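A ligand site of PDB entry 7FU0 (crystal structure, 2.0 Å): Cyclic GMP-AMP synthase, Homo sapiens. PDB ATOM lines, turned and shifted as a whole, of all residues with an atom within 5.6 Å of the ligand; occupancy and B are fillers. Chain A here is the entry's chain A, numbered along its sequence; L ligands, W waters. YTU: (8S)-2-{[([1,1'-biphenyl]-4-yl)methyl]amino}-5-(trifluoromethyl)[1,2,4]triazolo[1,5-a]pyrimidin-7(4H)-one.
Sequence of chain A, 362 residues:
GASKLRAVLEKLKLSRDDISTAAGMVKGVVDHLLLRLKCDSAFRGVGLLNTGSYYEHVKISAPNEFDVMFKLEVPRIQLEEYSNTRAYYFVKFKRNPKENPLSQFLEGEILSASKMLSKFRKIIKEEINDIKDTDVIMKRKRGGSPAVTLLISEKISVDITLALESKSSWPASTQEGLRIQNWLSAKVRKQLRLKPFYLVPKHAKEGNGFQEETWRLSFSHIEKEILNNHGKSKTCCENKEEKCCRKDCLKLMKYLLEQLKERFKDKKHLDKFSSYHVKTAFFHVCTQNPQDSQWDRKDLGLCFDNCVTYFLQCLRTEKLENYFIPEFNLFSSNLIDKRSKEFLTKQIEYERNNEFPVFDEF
OE2 of Glu 223 lies close to F26 of the ligand.
OG1 of Thr 280 sits close to F28 of the ligand.
Merely in contact with the ligand: Arg 216 (3.3 Å), Phe 283 (3.4 Å), Tyr 276 (3.5 Å), Phe 328 (3.5 Å), Lys 279 (3.5 Å), Ala 87 (3.5 Å), Ser 218 (3.6 Å), Ile 325 (3.6 Å), Phe 324 (3.7 Å), Leu 330 (3.8 Å) and Tyr 323 (3.8 Å).
Hydrophobic or aromatic side chains within 4 Å of the ligand: Ala 87, Phe 219, Tyr 276, Phe 283, Tyr 323, Phe 324, Ile 325, Phe 328 and Leu 330.
The side-chain amide oxygen (OD1) of Asn 322 lies within hydrogen-bond range of the backbone NH (N) of Phe 324, 2.7 Å away.
The backbone NH of Tyr 276 sits at hydrogen-bond distance from the side-chain hydroxyl of Ser 274, 3.0 Å away.
OD1 of Asn 322 lies within hydrogen-bond range of N of Ile 325 (2.9 Å).
The backbone carbonyl oxygen (O) of Tyr 276 lies within hydrogen-bond range of the side-chain hydroxyl (OG1) of Thr 280, 2.8 Å away.
O of Phe 328 sits at hydrogen-bond distance from N of Asn 322 (2.8 Å).
The backbone NH of Leu 217 is in hydrogen-bond range of the backbone carbonyl oxygen of Ala 87, 3.2 Å away.
The side-chain carboxylate (OE1) of Glu 223 lies within salt-bridge range of the side-chain amino group (NZ) of Lys 279 (2.7 Å).
The guanidinium group (NH2) of Arg 216 is in hydrogen-bond range of the side-chain hydroxyl (OH) of Tyr 88, at 3.0 Å.
A nitrogen (N14) of the ligand sits at hydrogen-bond distance from the backbone carbonyl oxygen (O) of Leu 217 (2.7 Å).
N of Phe 219 sits at hydrogen-bond distance from N16 of the ligand, at 3.0 Å.
ND2 of Asn 322 sits at hydrogen-bond distance from N24 of the ligand.
N of Ser 220 lies within hydrogen-bond range of O19 of the ligand.
Water W4 bridges the backbone carbonyl oxygen (O) of Leu 330 (2.7 Å) and a ring nitrogen (NE2) of His 277 (2.7 Å).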
ATOM      1  N   ALA A  87      -7.145 -10.776   7.784  1.00  0.00           N
ATOM      2  CA  ALA A  87      -7.789 -11.214   9.018  1.00  0.00           C
ATOM      3  C   ALA A  87      -8.986 -10.361   9.444  1.00  0.00           C
ATOM      4  O   ALA A  87      -9.779 -10.818  10.266  1.00  0.00           O
ATOM      5  CB  ALA A  87      -6.780 -11.208  10.172  1.00  0.00           C
ATOM      6  N   TYR A  88      -9.123  -9.138   8.931  1.00  0.00           N
ATOM      7  CA  TYR A  88     -10.178  -8.226   9.350  1.00  0.00           C
ATOM      8  C   TYR A  88     -11.236  -8.115   8.260  1.00  0.00           C
ATOM      9  O   TYR A  88     -10.911  -8.098   7.067  1.00  0.00           O
ATOM     10  CB  TYR A  88      -9.597  -6.862   9.724  1.00  0.00           C
ATOM     11  CG  TYR A  88      -8.651  -6.879  10.934  1.00  0.00           C
ATOM     12  CD1 TYR A  88      -7.322  -7.272  10.806  1.00  0.00           C
ATOM     13  CD2 TYR A  88      -9.099  -6.479  12.199  1.00  0.00           C
ATOM     14  CE1 TYR A  88      -6.467  -7.274  11.912  1.00  0.00           C
ATOM     15  CE2 TYR A  88      -8.258  -6.461  13.301  1.00  0.00           C
ATOM     16  CZ  TYR A  88      -6.934  -6.866  13.155  1.00  0.00           C
ATOM     17  OH  TYR A  88      -6.095  -6.882  14.272  1.00  0.00           O
ATOM     18  N   ARG A 216     -12.542  -9.492  13.356  1.00  0.00           N
ATOM     19  CA  ARG A 216     -11.350 -10.304  13.147  1.00  0.00           C
ATOM     20  C   ARG A 216     -11.683 -11.756  13.391  1.00  0.00           C
ATOM     21  O   ARG A 216     -12.428 -12.093  14.311  1.00  0.00           O
ATOM     22  CB  ARG A 216     -10.199  -9.863  14.092  1.00  0.00           C
ATOM     23  CG  ARG A 216      -8.910 -10.621  13.875  1.00  0.00           C
ATOM     24  CD  ARG A 216      -7.765  -9.923  14.611  1.00  0.00           C
ATOM     25  NE  ARG A 216      -7.653 -10.384  15.993  1.00  0.00           N
ATOM     26  CZ  ARG A 216      -6.931  -9.775  16.925  1.00  0.00           C
ATOM     27  NH1 ARG A 216      -6.880 -10.279  18.156  1.00  0.00           N
ATOM     28  NH2 ARG A 216      -6.270  -8.659  16.628  1.00  0.00           N
ATOM     29  N   LEU A 217     -11.110 -12.630  12.566  1.00  0.00           N
ATOM     30  CA  LEU A 217     -11.325 -14.056  12.733  1.00  0.00           C
ATOM     31  C   LEU A 217     -10.701 -14.530  14.043  1.00  0.00           C
ATOM     32  O   LEU A 217      -9.659 -14.030  14.465  1.00  0.00           O
ATOM     33  CB  LEU A 217     -10.723 -14.826  11.543  1.00  0.00           C
ATOM     34  CG  LEU A 217     -11.315 -14.568  10.157  1.00  0.00           C
ATOM     35  CD1 LEU A 217     -10.545 -15.323   9.034  1.00  0.00           C
ATOM     36  CD2 LEU A 217     -12.783 -14.978  10.145  1.00  0.00           C
ATOM     37  N   SER A 218     -11.365 -15.494  14.677  1.00  0.00           N
ATOM     38  CA  SER A 218     -10.932 -16.094  15.935  1.00  0.00           C
ATOM     39  C   SER A 218     -11.130 -17.582  15.830  1.00  0.00           C
ATOM     40  O   SER A 218     -12.222 -18.044  15.499  1.00  0.00           O
ATOM     41  CB  SER A 218     -11.746 -15.557  17.116  1.00  0.00           C
ATOM     42  OG  SER A 218     -11.593 -16.395  18.257  1.00  0.00           O
ATOM     43  N   PHE A 219     -10.081 -18.354  16.109  1.00  0.00           N
ATOM     44  CA  PHE A 219     -10.169 -19.809  16.022  1.00  0.00           C
ATOM     45  C   PHE A 219      -9.816 -20.475  17.356  1.00  0.00           C
ATOM     46  O   PHE A 219      -9.264 -21.571  17.378  1.00  0.00           O
ATOM     47  CB  PHE A 219      -9.287 -20.338  14.883  1.00  0.00           C
ATOM     48  CG  PHE A 219      -9.693 -19.832  13.520  1.00  0.00           C
ATOM     49  CD1 PHE A 219     -10.667 -20.479  12.791  1.00  0.00           C
ATOM     50  CD2 PHE A 219      -9.091 -18.700  12.976  1.00  0.00           C
ATOM     51  CE1 PHE A 219     -11.031 -20.030  11.511  1.00  0.00           C
ATOM     52  CE2 PHE A 219      -9.455 -18.223  11.711  1.00  0.00           C
ATOM     53  CZ  PHE A 219     -10.437 -18.891  10.981  1.00  0.00           C
ATOM     54  N   SER A 220     -10.121 -19.796  18.479  1.00  0.00           N
ATOM     55  CA  SER A 220      -9.688 -20.316  19.769  1.00  0.00           C
ATOM     56  C   SER A 220     -10.284 -21.699  20.052  1.00  0.00           C
ATOM     57  O   SER A 220      -9.666 -22.501  20.756  1.00  0.00           O
ATOM     58  CB  SER A 220     -10.063 -19.328  20.882  1.00  0.00           C
ATOM     59  OG  SER A 220     -11.455 -19.253  21.021  1.00  0.00           O
ATOM     60  N   HIS A 221     -11.446 -22.011  19.487  1.00  0.00           N
ATOM     61  CA  HIS A 221     -11.992 -23.349  19.666  1.00  0.00           C
ATOM     62  C   HIS A 221     -11.164 -24.394  18.930  1.00  0.00           C
ATOM     63  O   HIS A 221     -11.068 -25.530  19.389  1.00  0.00           O
ATOM     64  CB  HIS A 221     -13.435 -23.396  19.196  1.00  0.00           C
ATOM     65  CG  HIS A 221     -13.597 -23.060  17.747  1.00  0.00           C
ATOM     66  ND1 HIS A 221     -13.074 -21.909  17.185  1.00  0.00           N
ATOM     67  CD2 HIS A 221     -14.215 -23.730  16.746  1.00  0.00           C
ATOM     68  CE1 HIS A 221     -13.380 -21.879  15.899  1.00  0.00           C
ATOM     69  NE2 HIS A 221     -14.067 -22.973  15.601  1.00  0.00           N
ATOM     70  N   GLU A 223      -7.802 -24.141  18.231  1.00  0.00           N
ATOM     71  CA  GLU A 223      -6.621 -24.241  19.063  1.00  0.00           C
ATOM     72  C   GLU A 223      -6.870 -25.144  20.269  1.00  0.00           C
ATOM     73  O   GLU A 223      -6.041 -25.982  20.616  1.00  0.00           O
ATOM     74  CB  GLU A 223      -6.221 -22.844  19.521  1.00  0.00           C
ATOM     75  CG  GLU A 223      -5.431 -22.823  20.833  1.00  0.00           C
ATOM     76  CD  GLU A 223      -5.527 -21.484  21.524  1.00  0.00           C
ATOM     77  OE1 GLU A 223      -5.219 -21.399  22.723  1.00  0.00           O
ATOM     78  OE2 GLU A 223      -5.925 -20.508  20.857  1.00  0.00           O
ATOM     79  N   SER A 274       2.080 -11.118  23.026  1.00  0.00           N
ATOM     80  CA  SER A 274       1.037 -11.793  23.781  1.00  0.00           C
ATOM     81  C   SER A 274       1.123 -13.296  23.577  1.00  0.00           C
ATOM     82  O   SER A 274       1.906 -13.782  22.753  1.00  0.00           O
ATOM     83  CB  SER A 274      -0.354 -11.309  23.366  1.00  0.00           C
ATOM     84  OG  SER A 274      -0.819 -12.134  22.313  1.00  0.00           O
ATOM     85  N   SER A 275       0.267 -14.016  24.302  1.00  0.00           N
ATOM     86  CA  SER A 275       0.106 -15.465  24.132  1.00  0.00           C
ATOM     87  C   SER A 275      -0.039 -15.864  22.672  1.00  0.00           C
ATOM     88  O   SER A 275       0.423 -16.940  22.281  1.00  0.00           O
ATOM     89  CB  SER A 275      -1.120 -15.952  24.904  1.00  0.00           C
ATOM     90  OG  SER A 275      -0.755 -16.212  26.240  1.00  0.00           O
ATOM     91  N   TYR A 276      -0.717 -15.049  21.847  1.00  0.00           N
ATOM     92  CA  TYR A 276      -0.846 -15.381  20.427  1.00  0.00           C
ATOM     93  C   TYR A 276       0.508 -15.734  19.841  1.00  0.00           C
ATOM     94  O   TYR A 276       0.655 -16.757  19.169  1.00  0.00           O
ATOM     95  CB  TYR A 276      -1.446 -14.208  19.638  1.00  0.00           C
ATOM     96  CG  TYR A 276      -2.953 -14.204  19.505  1.00  0.00           C
ATOM     97  CD1 TYR A 276      -3.757 -13.587  20.454  1.00  0.00           C
ATOM     98  CD2 TYR A 276      -3.568 -14.815  18.409  1.00  0.00           C
ATOM     99  CE1 TYR A 276      -5.133 -13.578  20.329  1.00  0.00           C
ATOM    100  CE2 TYR A 276      -4.947 -14.813  18.279  1.00  0.00           C
ATOM    101  CZ  TYR A 276      -5.720 -14.197  19.246  1.00  0.00           C
ATOM    102  OH  TYR A 276      -7.097 -14.192  19.130  1.00  0.00           O
ATOM    103  N   HIS A 277       1.502 -14.895  20.089  1.00  0.00           N
ATOM    104  CA  HIS A 277       2.781 -15.057  19.405  1.00  0.00           C
ATOM    105  C   HIS A 277       3.470 -16.352  19.835  1.00  0.00           C
ATOM    106  O   HIS A 277       4.090 -17.028  19.001  1.00  0.00           O
ATOM    107  CB  HIS A 277       3.677 -13.845  19.660  1.00  0.00           C
ATOM    108  CG  HIS A 277       3.063 -12.551  19.223  1.00  0.00           C
ATOM    109  ND1 HIS A 277       2.592 -11.611  20.117  1.00  0.00           N
ATOM    110  CD2 HIS A 277       2.829 -12.046  17.989  1.00  0.00           C
ATOM    111  CE1 HIS A 277       2.097 -10.581  19.447  1.00  0.00           C
ATOM    112  NE2 HIS A 277       2.222 -10.820  18.153  1.00  0.00           N
ATOM    113  N   LYS A 279       1.917 -19.115  21.227  1.00  0.00           N
ATOM    114  CA  LYS A 279       1.095 -20.219  20.711  1.00  0.00           C
ATOM    115  C   LYS A 279       1.317 -20.430  19.233  1.00  0.00           C
ATOM    116  O   LYS A 279       1.439 -21.573  18.769  1.00  0.00           O
ATOM    117  CB  LYS A 279      -0.390 -19.950  20.980  1.00  0.00           C
ATOM    118  CG  LYS A 279      -0.806 -19.954  22.451  1.00  0.00           C
ATOM    119  CD  LYS A 279      -2.311 -19.652  22.560  1.00  0.00           C
ATOM    120  CE  LYS A 279      -2.729 -19.285  23.976  1.00  0.00           C
ATOM    121  NZ  LYS A 279      -4.228 -19.371  24.144  1.00  0.00           N
ATOM    122  N   THR A 280       1.394 -19.343  18.461  1.00  0.00           N
ATOM    123  CA  THR A 280       1.613 -19.479  17.024  1.00  0.00           C
ATOM    124  C   THR A 280       2.952 -20.142  16.742  1.00  0.00           C
ATOM    125  O   THR A 280       3.026 -21.131  16.003  1.00  0.00           O
ATOM    126  CB  THR A 280       1.541 -18.119  16.332  1.00  0.00           C
ATOM    127  OG1 THR A 280       0.227 -17.555  16.497  1.00  0.00           O
ATOM    128  CG2 THR A 280       1.844 -18.262  14.851  1.00  0.00           C
ATOM    129  N   PHE A 283       2.876 -23.887  17.536  1.00  0.00           N
ATOM    130  CA  PHE A 283       2.209 -24.736  16.554  1.00  0.00           C
ATOM    131  C   PHE A 283       3.040 -24.854  15.290  1.00  0.00           C
ATOM    132  O   PHE A 283       2.999 -25.889  14.619  1.00  0.00           O
ATOM    133  CB  PHE A 283       0.817 -24.199  16.213  1.00  0.00           C
ATOM    134  CG  PHE A 283      -0.211 -24.437  17.277  1.00  0.00           C
ATOM    135  CD1 PHE A 283      -0.407 -25.712  17.807  1.00  0.00           C
ATOM    136  CD2 PHE A 283      -0.976 -23.395  17.758  1.00  0.00           C
ATOM    137  CE1 PHE A 283      -1.339 -25.925  18.789  1.00  0.00           C
ATOM    138  CE2 PHE A 283      -1.930 -23.609  18.735  1.00  0.00           C
ATOM    139  CZ  PHE A 283      -2.120 -24.866  19.253  1.00  0.00           C
ATOM    140  N   ASN A 322       0.644 -16.027  11.075  1.00  0.00           N
ATOM    141  CA  ASN A 322      -0.493 -16.587  11.768  1.00  0.00           C
ATOM    142  C   ASN A 322      -0.705 -18.027  11.316  1.00  0.00           C
ATOM    143  O   ASN A 322      -0.569 -18.345  10.143  1.00  0.00           O
ATOM    144  CB  ASN A 322      -1.744 -15.753  11.479  1.00  0.00           C
ATOM    145  CG  ASN A 322      -2.955 -16.257  12.210  1.00  0.00           C
ATOM    146  OD1 ASN A 322      -3.647 -17.145  11.723  1.00  0.00           O
ATOM    147  ND2 ASN A 322      -3.211 -15.697  13.372  1.00  0.00           N
ATOM    148  N   TYR A 323      -1.020 -18.902  12.279  1.00  0.00           N
ATOM    149  CA  TYR A 323      -1.140 -20.329  11.968  1.00  0.00           C
ATOM    150  C   TYR A 323      -2.330 -20.627  11.081  1.00  0.00           C
ATOM    151  O   TYR A 323      -2.323 -21.623  10.336  1.00  0.00           O
ATOM    152  CB  TYR A 323      -1.262 -21.130  13.267  1.00  0.00           C
ATOM    153  CG  TYR A 323      -0.939 -22.607  13.128  1.00  0.00           C
ATOM    154  CD1 TYR A 323       0.337 -23.023  12.792  1.00  0.00           C
ATOM    155  CD2 TYR A 323      -1.926 -23.568  13.347  1.00  0.00           C
ATOM    156  CE1 TYR A 323       0.627 -24.367  12.660  1.00  0.00           C
ATOM    157  CE2 TYR A 323      -1.633 -24.905  13.243  1.00  0.00           C
ATOM    158  CZ  TYR A 323      -0.372 -25.304  12.889  1.00  0.00           C
ATOM    159  OH  TYR A 323      -0.121 -26.639  12.788  1.00  0.00           O
ATOM    160  N   PHE A 324      -3.383 -19.815  11.157  1.00  0.00           N
ATOM    161  CA  PHE A 324      -4.575 -20.065  10.353  1.00  0.00           C
ATOM    162  C   PHE A 324      -4.586 -19.273   9.056  1.00  0.00           C
ATOM    163  O   PHE A 324      -5.197 -19.711   8.077  1.00  0.00           O
ATOM    164  CB  PHE A 324      -5.840 -19.762  11.162  1.00  0.00           C
ATOM    165  CG  PHE A 324      -6.047 -20.693  12.326  1.00  0.00           C
ATOM    166  CD1 PHE A 324      -5.360 -20.497  13.503  1.00  0.00           C
ATOM    167  CD2 PHE A 324      -6.895 -21.761  12.228  1.00  0.00           C
ATOM    168  CE1 PHE A 324      -5.519 -21.335  14.566  1.00  0.00           C
ATOM    169  CE2 PHE A 324      -7.053 -22.625  13.312  1.00  0.00           C
ATOM    170  CZ  PHE A 324      -6.369 -22.408  14.477  1.00  0.00           C
ATOM    171  N   ILE A 325      -3.895 -18.139   9.029  1.00  0.00           N
ATOM    172  CA  ILE A 325      -3.906 -17.214   7.896  1.00  0.00           C
ATOM    173  C   ILE A 325      -2.442 -16.971   7.540  1.00  0.00           C
ATOM    174  O   ILE A 325      -1.830 -16.040   8.069  1.00  0.00           O
ATOM    175  CB  ILE A 325      -4.648 -15.922   8.263  1.00  0.00           C
ATOM    176  CG1 ILE A 325      -5.984 -16.280   8.919  1.00  0.00           C
ATOM    177  CG2 ILE A 325      -4.903 -15.067   7.040  1.00  0.00           C
ATOM    178  CD1 ILE A 325      -6.817 -15.083   9.354  1.00  0.00           C
ATOM    179  N   PHE A 328      -0.808 -13.453   7.081  1.00  0.00           N
ATOM    180  CA  PHE A 328      -0.775 -12.441   8.132  1.00  0.00           C
ATOM    181  C   PHE A 328       0.502 -12.622   8.953  1.00  0.00           C
ATOM    182  O   PHE A 328       0.672 -13.630   9.658  1.00  0.00           O
ATOM    183  CB  PHE A 328      -2.017 -12.510   9.022  1.00  0.00           C
ATOM    184  CG  PHE A 328      -2.178 -11.281   9.872  1.00  0.00           C
ATOM    185  CD1 PHE A 328      -1.488 -11.159  11.066  1.00  0.00           C
ATOM    186  CD2 PHE A 328      -2.965 -10.231   9.439  1.00  0.00           C
ATOM    187  CE1 PHE A 328      -1.611 -10.023  11.839  1.00  0.00           C
ATOM    188  CE2 PHE A 328      -3.089  -9.070  10.213  1.00  0.00           C
ATOM    189  CZ  PHE A 328      -2.398  -8.969  11.420  1.00  0.00           C
ATOM    190  N   LEU A 330       2.428 -11.746  11.950  1.00  0.00           N
ATOM    191  CA  LEU A 330       2.271 -11.184  13.284  1.00  0.00           C
ATOM    192  C   LEU A 330       3.433 -10.305  13.682  1.00  0.00           C
ATOM    193  O   LEU A 330       3.254  -9.442  14.549  1.00  0.00           O
ATOM    194  CB  LEU A 330       2.112 -12.318  14.303  1.00  0.00           C
ATOM    195  CG  LEU A 330       0.851 -13.122  14.110  1.00  0.00           C
ATOM    196  CD1 LEU A 330       0.915 -14.397  14.950  1.00  0.00           C
ATOM    197  CD2 LEU A 330      -0.354 -12.236  14.506  1.00  0.00           C
ATOM    198  N   LEU A 335       3.166  -3.918  12.971  1.00  0.00           N
ATOM    199  CA  LEU A 335       2.510  -4.360  14.200  1.00  0.00           C
ATOM    200  C   LEU A 335       3.427  -4.288  15.405  1.00  0.00           C
ATOM    201  O   LEU A 335       3.001  -3.885  16.491  1.00  0.00           O
ATOM    202  CB  LEU A 335       1.975  -5.775  14.016  1.00  0.00           C
ATOM    203  CG  LEU A 335       0.853  -6.034  13.002  1.00  0.00           C
ATOM    204  CD1 LEU A 335       0.547  -7.525  12.952  1.00  0.00           C
ATOM    205  CD2 LEU A 335      -0.419  -5.261  13.323  1.00  0.00           C
HETATM  206  C10 YTU L   1      -1.994  -8.694  17.135  1.00  0.00           C
HETATM  207  C11 YTU L   1      -2.632  -9.729  17.805  1.00  0.00           C
HETATM  208  C13 YTU L   1      -6.688 -14.745  12.917  1.00  0.00           C
HETATM  209  C15 YTU L   1      -6.824 -16.342  14.800  1.00  0.00           C
HETATM  210  C18 YTU L   1      -6.623 -18.478  17.585  1.00  0.00           C
HETATM  211  C20 YTU L   1      -5.407 -19.131  17.965  1.00  0.00           C
HETATM  212  C21 YTU L   1      -4.287 -18.989  17.274  1.00  0.00           C
HETATM  213  C23 YTU L   1      -5.285 -17.566  15.703  1.00  0.00           C
HETATM  214  C25 YTU L   1      -3.011 -19.653  17.752  1.00  0.00           C
HETATM  215  C1  YTU L   1      -5.113 -12.697  12.912  1.00  0.00           C
HETATM  216  C12 YTU L   1      -3.411 -10.643  17.100  1.00  0.00           C
HETATM  217  C2  YTU L   1      -5.884 -13.634  13.630  1.00  0.00           C
HETATM  218  C3  YTU L   1      -5.889 -13.499  15.031  1.00  0.00           C
HETATM  219  C4  YTU L   1      -5.131 -12.528  15.682  1.00  0.00           C
HETATM  220  C5  YTU L   1      -4.386 -11.577  14.977  1.00  0.00           C
HETATM  221  C6  YTU L   1      -4.373 -11.692  13.577  1.00  0.00           C
HETATM  222  C7  YTU L   1      -3.583 -10.548  15.704  1.00  0.00           C
HETATM  223  C8  YTU L   1      -2.897  -9.529  15.047  1.00  0.00           C
HETATM  224  C9  YTU L   1      -2.140  -8.587  15.763  1.00  0.00           C
HETATM  225  F26 YTU L   1      -3.268 -20.416  18.858  1.00  0.00           F
HETATM  226  F27 YTU L   1      -2.463 -20.428  16.825  1.00  0.00           F
HETATM  227  F28 YTU L   1      -2.059 -18.760  18.101  1.00  0.00           F
HETATM  228  N14 YTU L   1      -7.446 -15.438  13.954  1.00  0.00           N
HETATM  229  N16 YTU L   1      -7.473 -16.949  15.849  1.00  0.00           N
HETATM  230  N17 YTU L   1      -6.480 -17.704  16.415  1.00  0.00           N
HETATM  231  N22 YTU L   1      -4.147 -18.224  16.121  1.00  0.00           N
HETATM  232  N24 YTU L   1      -5.446 -16.718  14.670  1.00  0.00           N
HETATM  233  O19 YTU L   1      -7.657 -18.511  18.204  1.00  0.00           O
HETATM  234  O   HOH W   1      -1.728 -18.090  14.845  1.00  0.00           O
HETATM  235  O   HOH W   2      -4.881  -8.048  19.519  1.00  0.00           O
HETATM  236  O   HOH W   3      -2.568  -9.416  20.970  1.00  0.00           O
HETATM  237  O   HOH W   4       1.311  -8.987  16.349  1.00  0.00           O
